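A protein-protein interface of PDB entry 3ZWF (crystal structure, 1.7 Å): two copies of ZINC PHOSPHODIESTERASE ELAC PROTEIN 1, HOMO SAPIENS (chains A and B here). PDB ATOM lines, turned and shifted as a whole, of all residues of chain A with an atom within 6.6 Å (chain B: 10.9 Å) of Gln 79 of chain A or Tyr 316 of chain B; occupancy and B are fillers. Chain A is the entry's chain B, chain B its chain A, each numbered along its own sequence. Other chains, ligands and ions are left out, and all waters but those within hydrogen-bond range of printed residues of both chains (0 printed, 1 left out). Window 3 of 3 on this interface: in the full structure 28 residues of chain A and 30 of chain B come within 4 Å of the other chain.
Hydrophobic or aromatic side chains of chain A within 4 Å of the printed part of chain B: Met 44 and Leu 78. Of the 18 printed residues of chain B, 6 touch a printed residue of chain A. Hydrophobic or aromatic side chains of chain B that line the printed part of chain A: Tyr 12, Pro 15 and Tyr 316. Among the printed residues, 7 pairs touch across the chains.
OH of Tyr 12 of chain B lies within hydrogen-bond range of NE2 of Gln 79 of chain A (3.2 Å). The backbone carbonyl oxygen (O) of Pro 13 of chain B sits close to the side-chain sulfur (SD) of Met 44 of chain A (3.6 Å).
Gln 79 of chain A touches just these residues of chain B: Tyr 12 (3.2 Å) and Tyr 316 (3.5 Å). Tyr 316 of chain B touches one residue of chain A. No residue of chain B comes within 4 Å of Ser 77 of chain A. Leu 78 of chain A touches one residue of chain B. Of the printed residues of chain B, Met 44 of chain A touches Pro 13 (3.6 Å), Ser 14 (3.7 Å) and Pro 15 (3.6 Å). Printed residues of chain A within 4 Å of Pro 15 of chain B: Met 44 (3.6 Å). Printed residues of chain A within 4 Å of Ala 11 of chain B: Leu 78 (3.9 Å). Of the printed residues of chain A, Ser 14 of chain B touches Met 44 (3.7 Å). Of the printed residues of chain A, Pro 13 of chain B touches Met 44. The nearest printed residue of chain B that does not touch Thr 75 of chain A is Ala 11 of chain B (5.0 Å).
Ser 14 of chain B touches Met 44 of chain A (CB to CE, 3.7 Å). Met 44 of chain A touches Pro 15 of chain B. OG1 of Thr 75 of chain A touches CB of Tyr 12 of chain B (3.3 Å). Leu 78 of chain A touches Ala 11 of chain B (CD1 to O, 3.9 Å). O of Gln 79 of chain A touches OH of Tyr 316 of chain B, 3.5 Å away.
No position is printed for both chains. Of the 7 pairs that touch across the chains among the printed residues, none has its exchanged pair printed and touching as well.
The backbone carbonyl oxygen of Tyr 12 of chain B sits at hydrogen-bond distance from the side-chain amide nitrogen of Gln 314 of chain B. The side-chain hydroxyl (OG1) of Thr 16 of chain B sits at hydrogen-bond distance from the side-chain hydroxyl (OG) of Ser 14 of chain B (3.2 Å). The side-chain hydroxyl of Ser 14 of chain B is in hydrogen-bond range of the backbone NH of Arg 17 of chain B (3.1 Å). OG of Ser 14 of chain B sits at hydrogen-bond distance from OE1 of Gln 314 of chain B (2.7 Å).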
ATOM      1  N   MET A  44     -14.892 -23.796 -13.910  1.00  0.00           N
ATOM      2  CA  MET A  44     -16.097 -24.189 -13.255  1.00  0.00           C
ATOM      3  C   MET A  44     -15.832 -25.289 -12.208  1.00  0.00           C
ATOM      4  O   MET A  44     -16.421 -25.273 -11.132  1.00  0.00           O
ATOM      5  CB  MET A  44     -17.191 -24.596 -14.273  1.00  0.00           C
ATOM      6  CG  MET A  44     -17.543 -23.452 -15.097  1.00  0.00           C
ATOM      7  SD  MET A  44     -18.671 -24.129 -16.374  1.00  0.00           S
ATOM      8  CE  MET A  44     -20.021 -24.450 -15.304  1.00  0.00           C
ATOM      9  N   LYS A  49     -13.703 -18.510  -9.709  1.00  0.00           N
ATOM     10  CA  LYS A  49     -14.899 -18.067 -10.437  1.00  0.00           C
ATOM     11  C   LYS A  49     -14.466 -17.183 -11.588  1.00  0.00           C
ATOM     12  O   LYS A  49     -13.709 -16.212 -11.387  1.00  0.00           O
ATOM     13  CB  LYS A  49     -15.869 -17.315  -9.514  1.00  0.00           C
ATOM     14  CG  LYS A  49     -16.585 -18.192  -8.465  1.00  0.00           C
ATOM     15  CD  LYS A  49     -17.895 -18.742  -8.947  1.00  0.00           C
ATOM     16  CE  LYS A  49     -18.575 -19.587  -7.862  1.00  0.00           C
ATOM     17  N   ALA A  50     -14.924 -17.534 -12.792  1.00  0.00           N
ATOM     18  CA  ALA A  50     -14.577 -16.790 -14.020  1.00  0.00           C
ATOM     19  C   ALA A  50     -14.847 -15.299 -13.886  1.00  0.00           C
ATOM     20  O   ALA A  50     -14.058 -14.457 -14.365  1.00  0.00           O
ATOM     21  CB  ALA A  50     -15.331 -17.355 -15.221  1.00  0.00           C
ATOM     22  N   GLY A  51     -15.919 -14.966 -13.180  1.00  0.00           N
ATOM     23  CA  GLY A  51     -16.322 -13.570 -12.948  1.00  0.00           C
ATOM     24  C   GLY A  51     -15.340 -12.693 -12.199  1.00  0.00           C
ATOM     25  O   GLY A  51     -15.442 -11.468 -12.251  1.00  0.00           O
ATOM     26  N   CYS A  74     -17.414 -15.105 -23.380  1.00  0.00           N
ATOM     27  CA  CYS A  74     -18.874 -15.220 -23.572  1.00  0.00           C
ATOM     28  C   CYS A  74     -19.564 -15.663 -22.298  1.00  0.00           C
ATOM     29  O   CYS A  74     -20.605 -15.142 -21.907  1.00  0.00           O
ATOM     30  CB  CYS A  74     -19.195 -16.213 -24.709  1.00  0.00           C
ATOM     31  SG  CYS A  74     -18.870 -15.637 -26.254  1.00  0.00           S
ATOM     32  N   THR A  75     -18.984 -16.655 -21.666  1.00  0.00           N
ATOM     33  CA  THR A  75     -19.567 -17.276 -20.483  1.00  0.00           C
ATOM     34  C   THR A  75     -19.504 -16.303 -19.302  1.00  0.00           C
ATOM     35  O   THR A  75     -20.481 -16.156 -18.573  1.00  0.00           O
ATOM     36  CB  THR A  75     -18.914 -18.665 -20.244  1.00  0.00           C
ATOM     37  OG1 THR A  75     -19.255 -19.493 -21.382  1.00  0.00           O
ATOM     38  CG2 THR A  75     -19.384 -19.311 -18.928  1.00  0.00           C
ATOM     39  N   ILE A  76     -18.369 -15.605 -19.152  1.00  0.00           N
ATOM     40  CA  ILE A  76     -18.283 -14.530 -18.138  1.00  0.00           C
ATOM     41  C   ILE A  76     -19.432 -13.516 -18.350  1.00  0.00           C
ATOM     42  O   ILE A  76     -20.132 -13.133 -17.417  1.00  0.00           O
ATOM     43  CB  ILE A  76     -16.946 -13.797 -18.178  1.00  0.00           C
ATOM     44  CG1 ILE A  76     -15.820 -14.677 -17.660  1.00  0.00           C
ATOM     45  CG2 ILE A  76     -17.000 -12.448 -17.413  1.00  0.00           C
ATOM     46  CD1 ILE A  76     -14.487 -14.108 -17.974  1.00  0.00           C
ATOM     47  N   SER A  77     -19.662 -13.123 -19.591  1.00  0.00           N
ATOM     48  CA  SER A  77     -20.714 -12.156 -19.876  1.00  0.00           C
ATOM     49  C   SER A  77     -22.118 -12.738 -19.558  1.00  0.00           C
ATOM     50  O   SER A  77     -22.911 -12.111 -18.851  1.00  0.00           O
ATOM     51  CB  SER A  77     -20.654 -11.728 -21.306  1.00  0.00           C
ATOM     52  OG  SER A  77     -21.665 -10.773 -21.553  1.00  0.00           O
ATOM     53  N   LEU A  78     -22.397 -13.933 -20.091  1.00  0.00           N
ATOM     54  CA  LEU A  78     -23.696 -14.644 -19.891  1.00  0.00           C
ATOM     55  C   LEU A  78     -24.050 -14.772 -18.431  1.00  0.00           C
ATOM     56  O   LEU A  78     -25.235 -14.716 -18.044  1.00  0.00           O
ATOM     57  CB  LEU A  78     -23.670 -16.073 -20.465  1.00  0.00           C
ATOM     58  CG  LEU A  78     -23.905 -16.210 -21.973  1.00  0.00           C
ATOM     59  CD1 LEU A  78     -23.581 -17.636 -22.430  1.00  0.00           C
ATOM     60  CD2 LEU A  78     -25.321 -15.806 -22.366  1.00  0.00           C
ATOM     61  N   GLN A  79     -23.021 -14.980 -17.621  1.00  0.00           N
ATOM     62  CA  GLN A  79     -23.220 -15.219 -16.180  1.00  0.00           C
ATOM     63  C   GLN A  79     -23.081 -13.976 -15.275  1.00  0.00           C
ATOM     64  O   GLN A  79     -23.290 -14.084 -14.064  1.00  0.00           O
ATOM     65  CB  GLN A  79     -22.298 -16.352 -15.690  1.00  0.00           C
ATOM     66  CG  GLN A  79     -22.515 -17.716 -16.370  1.00  0.00           C
ATOM     67  CD  GLN A  79     -21.554 -18.780 -15.841  1.00  0.00           C
ATOM     68  OE1 GLN A  79     -20.463 -18.456 -15.387  1.00  0.00           O
ATOM     69  NE2 GLN A  79     -21.968 -20.041 -15.874  1.00  0.00           N
ATOM     70  N   SER A  80     -22.798 -12.807 -15.848  1.00  0.00           N
ATOM     71  CA  SER A  80     -22.483 -11.580 -15.051  1.00  0.00           C
ATOM     72  C   SER A  80     -23.568 -11.161 -14.048  1.00  0.00           C
ATOM     73  O   SER A  80     -24.704 -10.867 -14.426  1.00  0.00           O
ATOM     74  CB  SER A  80     -22.168 -10.388 -15.977  1.00  0.00           C
ATOM     75  N   GLY B   9     -25.789 -29.645 -23.307  1.00  0.00           N
ATOM     76  CA  GLY B   9     -26.147 -28.437 -22.613  1.00  0.00           C
ATOM     77  C   GLY B   9     -26.358 -27.234 -23.505  1.00  0.00           C
ATOM     78  O   GLY B   9     -25.808 -27.134 -24.637  1.00  0.00           O
ATOM     79  N   ALA B  10     -27.086 -26.274 -22.950  1.00  0.00           N
ATOM     80  CA  ALA B  10     -27.351 -24.968 -23.592  1.00  0.00           C
ATOM     81  C   ALA B  10     -26.316 -23.922 -23.270  1.00  0.00           C
ATOM     82  O   ALA B  10     -25.826 -23.862 -22.154  1.00  0.00           O
ATOM     83  CB  ALA B  10     -28.684 -24.423 -23.160  1.00  0.00           C
ATOM     84  N   ALA B  11     -25.996 -23.118 -24.281  1.00  0.00           N
ATOM     85  CA  ALA B  11     -25.276 -21.836 -24.171  1.00  0.00           C
ATOM     86  C   ALA B  11     -23.772 -21.864 -23.863  1.00  0.00           C
ATOM     87  O   ALA B  11     -23.052 -20.971 -24.311  1.00  0.00           O
ATOM     88  CB  ALA B  11     -26.029 -20.881 -23.215  1.00  0.00           C
ATOM     89  N   TYR B  12     -23.308 -22.837 -23.091  1.00  0.00           N
ATOM     90  CA  TYR B  12     -21.917 -23.034 -22.752  1.00  0.00           C
ATOM     91  C   TYR B  12     -21.690 -24.421 -22.235  1.00  0.00           C
ATOM     92  O   TYR B  12     -22.628 -25.071 -21.768  1.00  0.00           O
ATOM     93  CB  TYR B  12     -21.435 -22.012 -21.699  1.00  0.00           C
ATOM     94  CG  TYR B  12     -22.229 -21.980 -20.453  1.00  0.00           C
ATOM     95  CD1 TYR B  12     -23.351 -21.166 -20.329  1.00  0.00           C
ATOM     96  CD2 TYR B  12     -21.872 -22.782 -19.363  1.00  0.00           C
ATOM     97  CE1 TYR B  12     -24.039 -21.117 -19.161  1.00  0.00           C
ATOM     98  CE2 TYR B  12     -22.568 -22.750 -18.223  1.00  0.00           C
ATOM     99  CZ  TYR B  12     -23.655 -21.915 -18.112  1.00  0.00           C
ATOM    100  OH  TYR B  12     -24.353 -21.907 -16.920  1.00  0.00           O
ATOM    101  N   PRO B  13     -20.452 -24.900 -22.298  1.00  0.00           N
ATOM    102  CA  PRO B  13     -20.160 -26.213 -21.756  1.00  0.00           C
ATOM    103  C   PRO B  13     -20.045 -26.157 -20.263  1.00  0.00           C
ATOM    104  O   PRO B  13     -19.576 -25.154 -19.757  1.00  0.00           O
ATOM    105  CB  PRO B  13     -18.804 -26.538 -22.378  1.00  0.00           C
ATOM    106  CG  PRO B  13     -18.213 -25.252 -22.649  1.00  0.00           C
ATOM    107  CD  PRO B  13     -19.283 -24.297 -22.946  1.00  0.00           C
ATOM    108  N   SER B  14     -20.466 -27.218 -19.589  1.00  0.00           N
ATOM    109  CA  SER B  14     -20.263 -27.371 -18.140  1.00  0.00           C
ATOM    110  C   SER B  14     -19.690 -28.746 -17.847  1.00  0.00           C
ATOM    111  O   SER B  14     -19.580 -29.581 -18.739  1.00  0.00           O
ATOM    112  CB  SER B  14     -21.547 -27.153 -17.375  1.00  0.00           C
ATOM    113  OG  SER B  14     -22.370 -28.348 -17.426  1.00  0.00           O
ATOM    114  N   PRO B  15     -19.257 -28.964 -16.608  1.00  0.00           N
ATOM    115  CA  PRO B  15     -18.767 -30.270 -16.193  1.00  0.00           C
ATOM    116  C   PRO B  15     -19.813 -31.395 -16.328  1.00  0.00           C
ATOM    117  O   PRO B  15     -19.446 -32.550 -16.540  1.00  0.00           O
ATOM    118  CB  PRO B  15     -18.393 -30.056 -14.712  1.00  0.00           C
ATOM    119  CG  PRO B  15     -18.101 -28.611 -14.585  1.00  0.00           C
ATOM    120  CD  PRO B  15     -19.152 -27.974 -15.520  1.00  0.00           C
ATOM    121  N   THR B  16     -21.087 -31.046 -16.272  1.00  0.00           N
ATOM    122  CA  THR B  16     -22.167 -32.082 -16.365  1.00  0.00           C
ATOM    123  C   THR B  16     -22.782 -32.244 -17.744  1.00  0.00           C
ATOM    124  O   THR B  16     -23.298 -33.320 -18.087  1.00  0.00           O
ATOM    125  CB  THR B  16     -23.262 -31.796 -15.333  1.00  0.00           C
ATOM    126  OG1 THR B  16     -23.791 -30.487 -15.527  1.00  0.00           O
ATOM    127  CG2 THR B  16     -22.715 -31.858 -13.944  1.00  0.00           C
ATOM    128  N   ARG B  17     -22.747 -31.170 -18.534  1.00  0.00           N
ATOM    129  CA  ARG B  17     -23.242 -31.188 -19.924  1.00  0.00           C
ATOM    130  C   ARG B  17     -22.355 -30.342 -20.838  1.00  0.00           C
ATOM    131  O   ARG B  17     -22.271 -29.121 -20.666  1.00  0.00           O
ATOM    132  CB  ARG B  17     -24.681 -30.685 -20.047  1.00  0.00           C
ATOM    133  CG  ARG B  17     -25.763 -31.483 -19.335  1.00  0.00           C
ATOM    134  CD  ARG B  17     -27.128 -30.902 -19.657  1.00  0.00           C
ATOM    135  NE  ARG B  17     -28.267 -31.519 -18.958  1.00  0.00           N
ATOM    136  CZ  ARG B  17     -28.862 -32.651 -19.338  1.00  0.00           C
ATOM    137  NH1 ARG B  17     -28.422 -33.343 -20.384  1.00  0.00           N
ATOM    138  NH2 ARG B  17     -29.913 -33.092 -18.685  1.00  0.00           N
ATOM    139  N   THR B 275     -34.595 -25.938 -24.333  1.00  0.00           N
ATOM    140  CA  THR B 275     -33.710 -25.178 -23.439  1.00  0.00           C
ATOM    141  C   THR B 275     -34.309 -24.951 -22.051  1.00  0.00           C
ATOM    142  O   THR B 275     -33.635 -25.141 -21.017  1.00  0.00           O
ATOM    143  CB  THR B 275     -33.229 -23.839 -24.067  1.00  0.00           C
ATOM    144  OG1 THR B 275     -32.562 -24.105 -25.309  1.00  0.00           O
ATOM    145  CG2 THR B 275     -32.300 -23.125 -23.090  1.00  0.00           C
ATOM    146  N   LEU B 276     -35.595 -24.589 -22.015  1.00  0.00           N
ATOM    147  CA  LEU B 276     -36.256 -24.269 -20.770  1.00  0.00           C
ATOM    148  C   LEU B 276     -37.529 -25.097 -20.658  1.00  0.00           C
ATOM    149  O   LEU B 276     -38.033 -25.619 -21.650  1.00  0.00           O
ATOM    150  CB  LEU B 276     -36.644 -22.795 -20.716  1.00  0.00           C
ATOM    151  CG  LEU B 276     -35.508 -21.795 -20.715  1.00  0.00           C
ATOM    152  CD1 LEU B 276     -36.054 -20.376 -20.655  1.00  0.00           C
ATOM    153  CD2 LEU B 276     -34.655 -22.115 -19.492  1.00  0.00           C
ATOM    154  N   GLN B 280     -41.561 -21.594 -18.553  1.00  0.00           N
ATOM    155  CA  GLN B 280     -40.727 -20.453 -19.044  1.00  0.00           C
ATOM    156  C   GLN B 280     -40.779 -20.254 -20.555  1.00  0.00           C
ATOM    157  O   GLN B 280     -39.818 -19.760 -21.173  1.00  0.00           O
ATOM    158  CB  GLN B 280     -39.281 -20.631 -18.610  1.00  0.00           C
ATOM    159  CG  GLN B 280     -39.108 -20.853 -17.105  1.00  0.00           C
ATOM    160  CD  GLN B 280     -37.666 -20.729 -16.659  1.00  0.00           C
ATOM    161  OE1 GLN B 280     -37.011 -21.709 -16.311  1.00  0.00           O
ATOM    162  NE2 GLN B 280     -37.170 -19.529 -16.685  1.00  0.00           N
ATOM    163  N   LYS B 283     -39.952 -16.665 -21.832  1.00  0.00           N
ATOM    164  CA  LYS B 283     -38.519 -16.464 -21.811  1.00  0.00           C
ATOM    165  C   LYS B 283     -37.803 -17.259 -22.916  1.00  0.00           C
ATOM    166  O   LYS B 283     -36.914 -16.736 -23.597  1.00  0.00           O
ATOM    167  CB  LYS B 283     -37.922 -16.814 -20.456  1.00  0.00           C
ATOM    168  CG  LYS B 283     -36.436 -16.564 -20.378  1.00  0.00           C
ATOM    169  CD  LYS B 283     -35.918 -16.771 -18.947  1.00  0.00           C
ATOM    170  CE  LYS B 283     -34.478 -16.417 -18.830  1.00  0.00           C
ATOM    171  NZ  LYS B 283     -33.597 -17.399 -19.515  1.00  0.00           N
ATOM    172  N   PHE B 312     -30.241 -28.498 -22.974  1.00  0.00           N
ATOM    173  CA  PHE B 312     -30.852 -28.108 -21.729  1.00  0.00           C
ATOM    174  C   PHE B 312     -30.107 -27.007 -20.972  1.00  0.00           C
ATOM    175  O   PHE B 312     -28.897 -26.996 -20.941  1.00  0.00           O
ATOM    176  CB  PHE B 312     -30.962 -29.329 -20.817  1.00  0.00           C
ATOM    177  CG  PHE B 312     -31.794 -30.464 -21.382  1.00  0.00           C
ATOM    178  CD1 PHE B 312     -33.153 -30.323 -21.483  1.00  0.00           C
ATOM    179  CD2 PHE B 312     -31.201 -31.666 -21.774  1.00  0.00           C
ATOM    180  CE1 PHE B 312     -33.917 -31.347 -22.025  1.00  0.00           C
ATOM    181  CE2 PHE B 312     -31.951 -32.704 -22.313  1.00  0.00           C
ATOM    182  CZ  PHE B 312     -33.313 -32.561 -22.397  1.00  0.00           C
ATOM    183  N   SER B 313     -30.871 -26.051 -20.448  1.00  0.00           N
ATOM    184  CA  SER B 313     -30.337 -25.003 -19.602  1.00  0.00           C
ATOM    185  C   SER B 313     -29.413 -25.632 -18.540  1.00  0.00           C
ATOM    186  O   SER B 313     -29.737 -26.670 -17.921  1.00  0.00           O
ATOM    187  CB  SER B 313     -31.470 -24.223 -18.920  1.00  0.00           C
ATOM    188  OG  SER B 313     -30.933 -23.239 -18.029  1.00  0.00           O
ATOM    189  N   GLN B 314     -28.257 -24.972 -18.352  1.00  0.00           N
ATOM    190  CA  GLN B 314     -27.267 -25.485 -17.413  1.00  0.00           C
ATOM    191  C   GLN B 314     -27.705 -25.183 -15.962  1.00  0.00           C
ATOM    192  O   GLN B 314     -28.449 -24.238 -15.696  1.00  0.00           O
ATOM    193  CB  GLN B 314     -25.893 -24.870 -17.687  1.00  0.00           C
ATOM    194  CG  GLN B 314     -25.233 -25.262 -18.967  1.00  0.00           C
ATOM    195  CD  GLN B 314     -24.620 -26.651 -19.002  1.00  0.00           C
ATOM    196  OE1 GLN B 314     -24.813 -27.471 -18.100  1.00  0.00           O
ATOM    197  NE2 GLN B 314     -23.902 -26.939 -20.104  1.00  0.00           N
ATOM    198  N   ARG B 315     -27.250 -26.022 -15.041  1.00  0.00           N
ATOM    199  CA  ARG B 315     -27.536 -25.832 -13.623  1.00  0.00           C
ATOM    200  C   ARG B 315     -26.575 -24.737 -13.169  1.00  0.00           C
ATOM    201  O   ARG B 315     -25.444 -25.026 -12.782  1.00  0.00           O
ATOM    202  CB  ARG B 315     -27.325 -27.133 -12.832  1.00  0.00           C
ATOM    203  N   TYR B 316     -27.007 -23.481 -13.315  1.00  0.00           N
ATOM    204  CA  TYR B 316     -26.257 -22.308 -12.828  1.00  0.00           C
ATOM    205  C   TYR B 316     -27.126 -21.439 -11.912  1.00  0.00           C
ATOM    206  O   TYR B 316     -27.537 -20.333 -12.282  1.00  0.00           O
ATOM    207  CB  TYR B 316     -25.703 -21.454 -13.984  1.00  0.00           C
ATOM    208  CG  TYR B 316     -24.950 -20.230 -13.479  1.00  0.00           C
ATOM    209  CD1 TYR B 316     -23.806 -20.379 -12.695  1.00  0.00           C
ATOM    210  CD2 TYR B 316     -25.406 -18.934 -13.742  1.00  0.00           C
ATOM    211  CE1 TYR B 316     -23.118 -19.271 -12.201  1.00  0.00           C
ATOM    212  CE2 TYR B 316     -24.732 -17.817 -13.253  1.00  0.00           C
ATOM    213  CZ  TYR B 316     -23.584 -17.997 -12.479  1.00  0.00           C
ATOM    214  OH  TYR B 316     -22.898 -16.922 -11.979  1.00  0.00           O
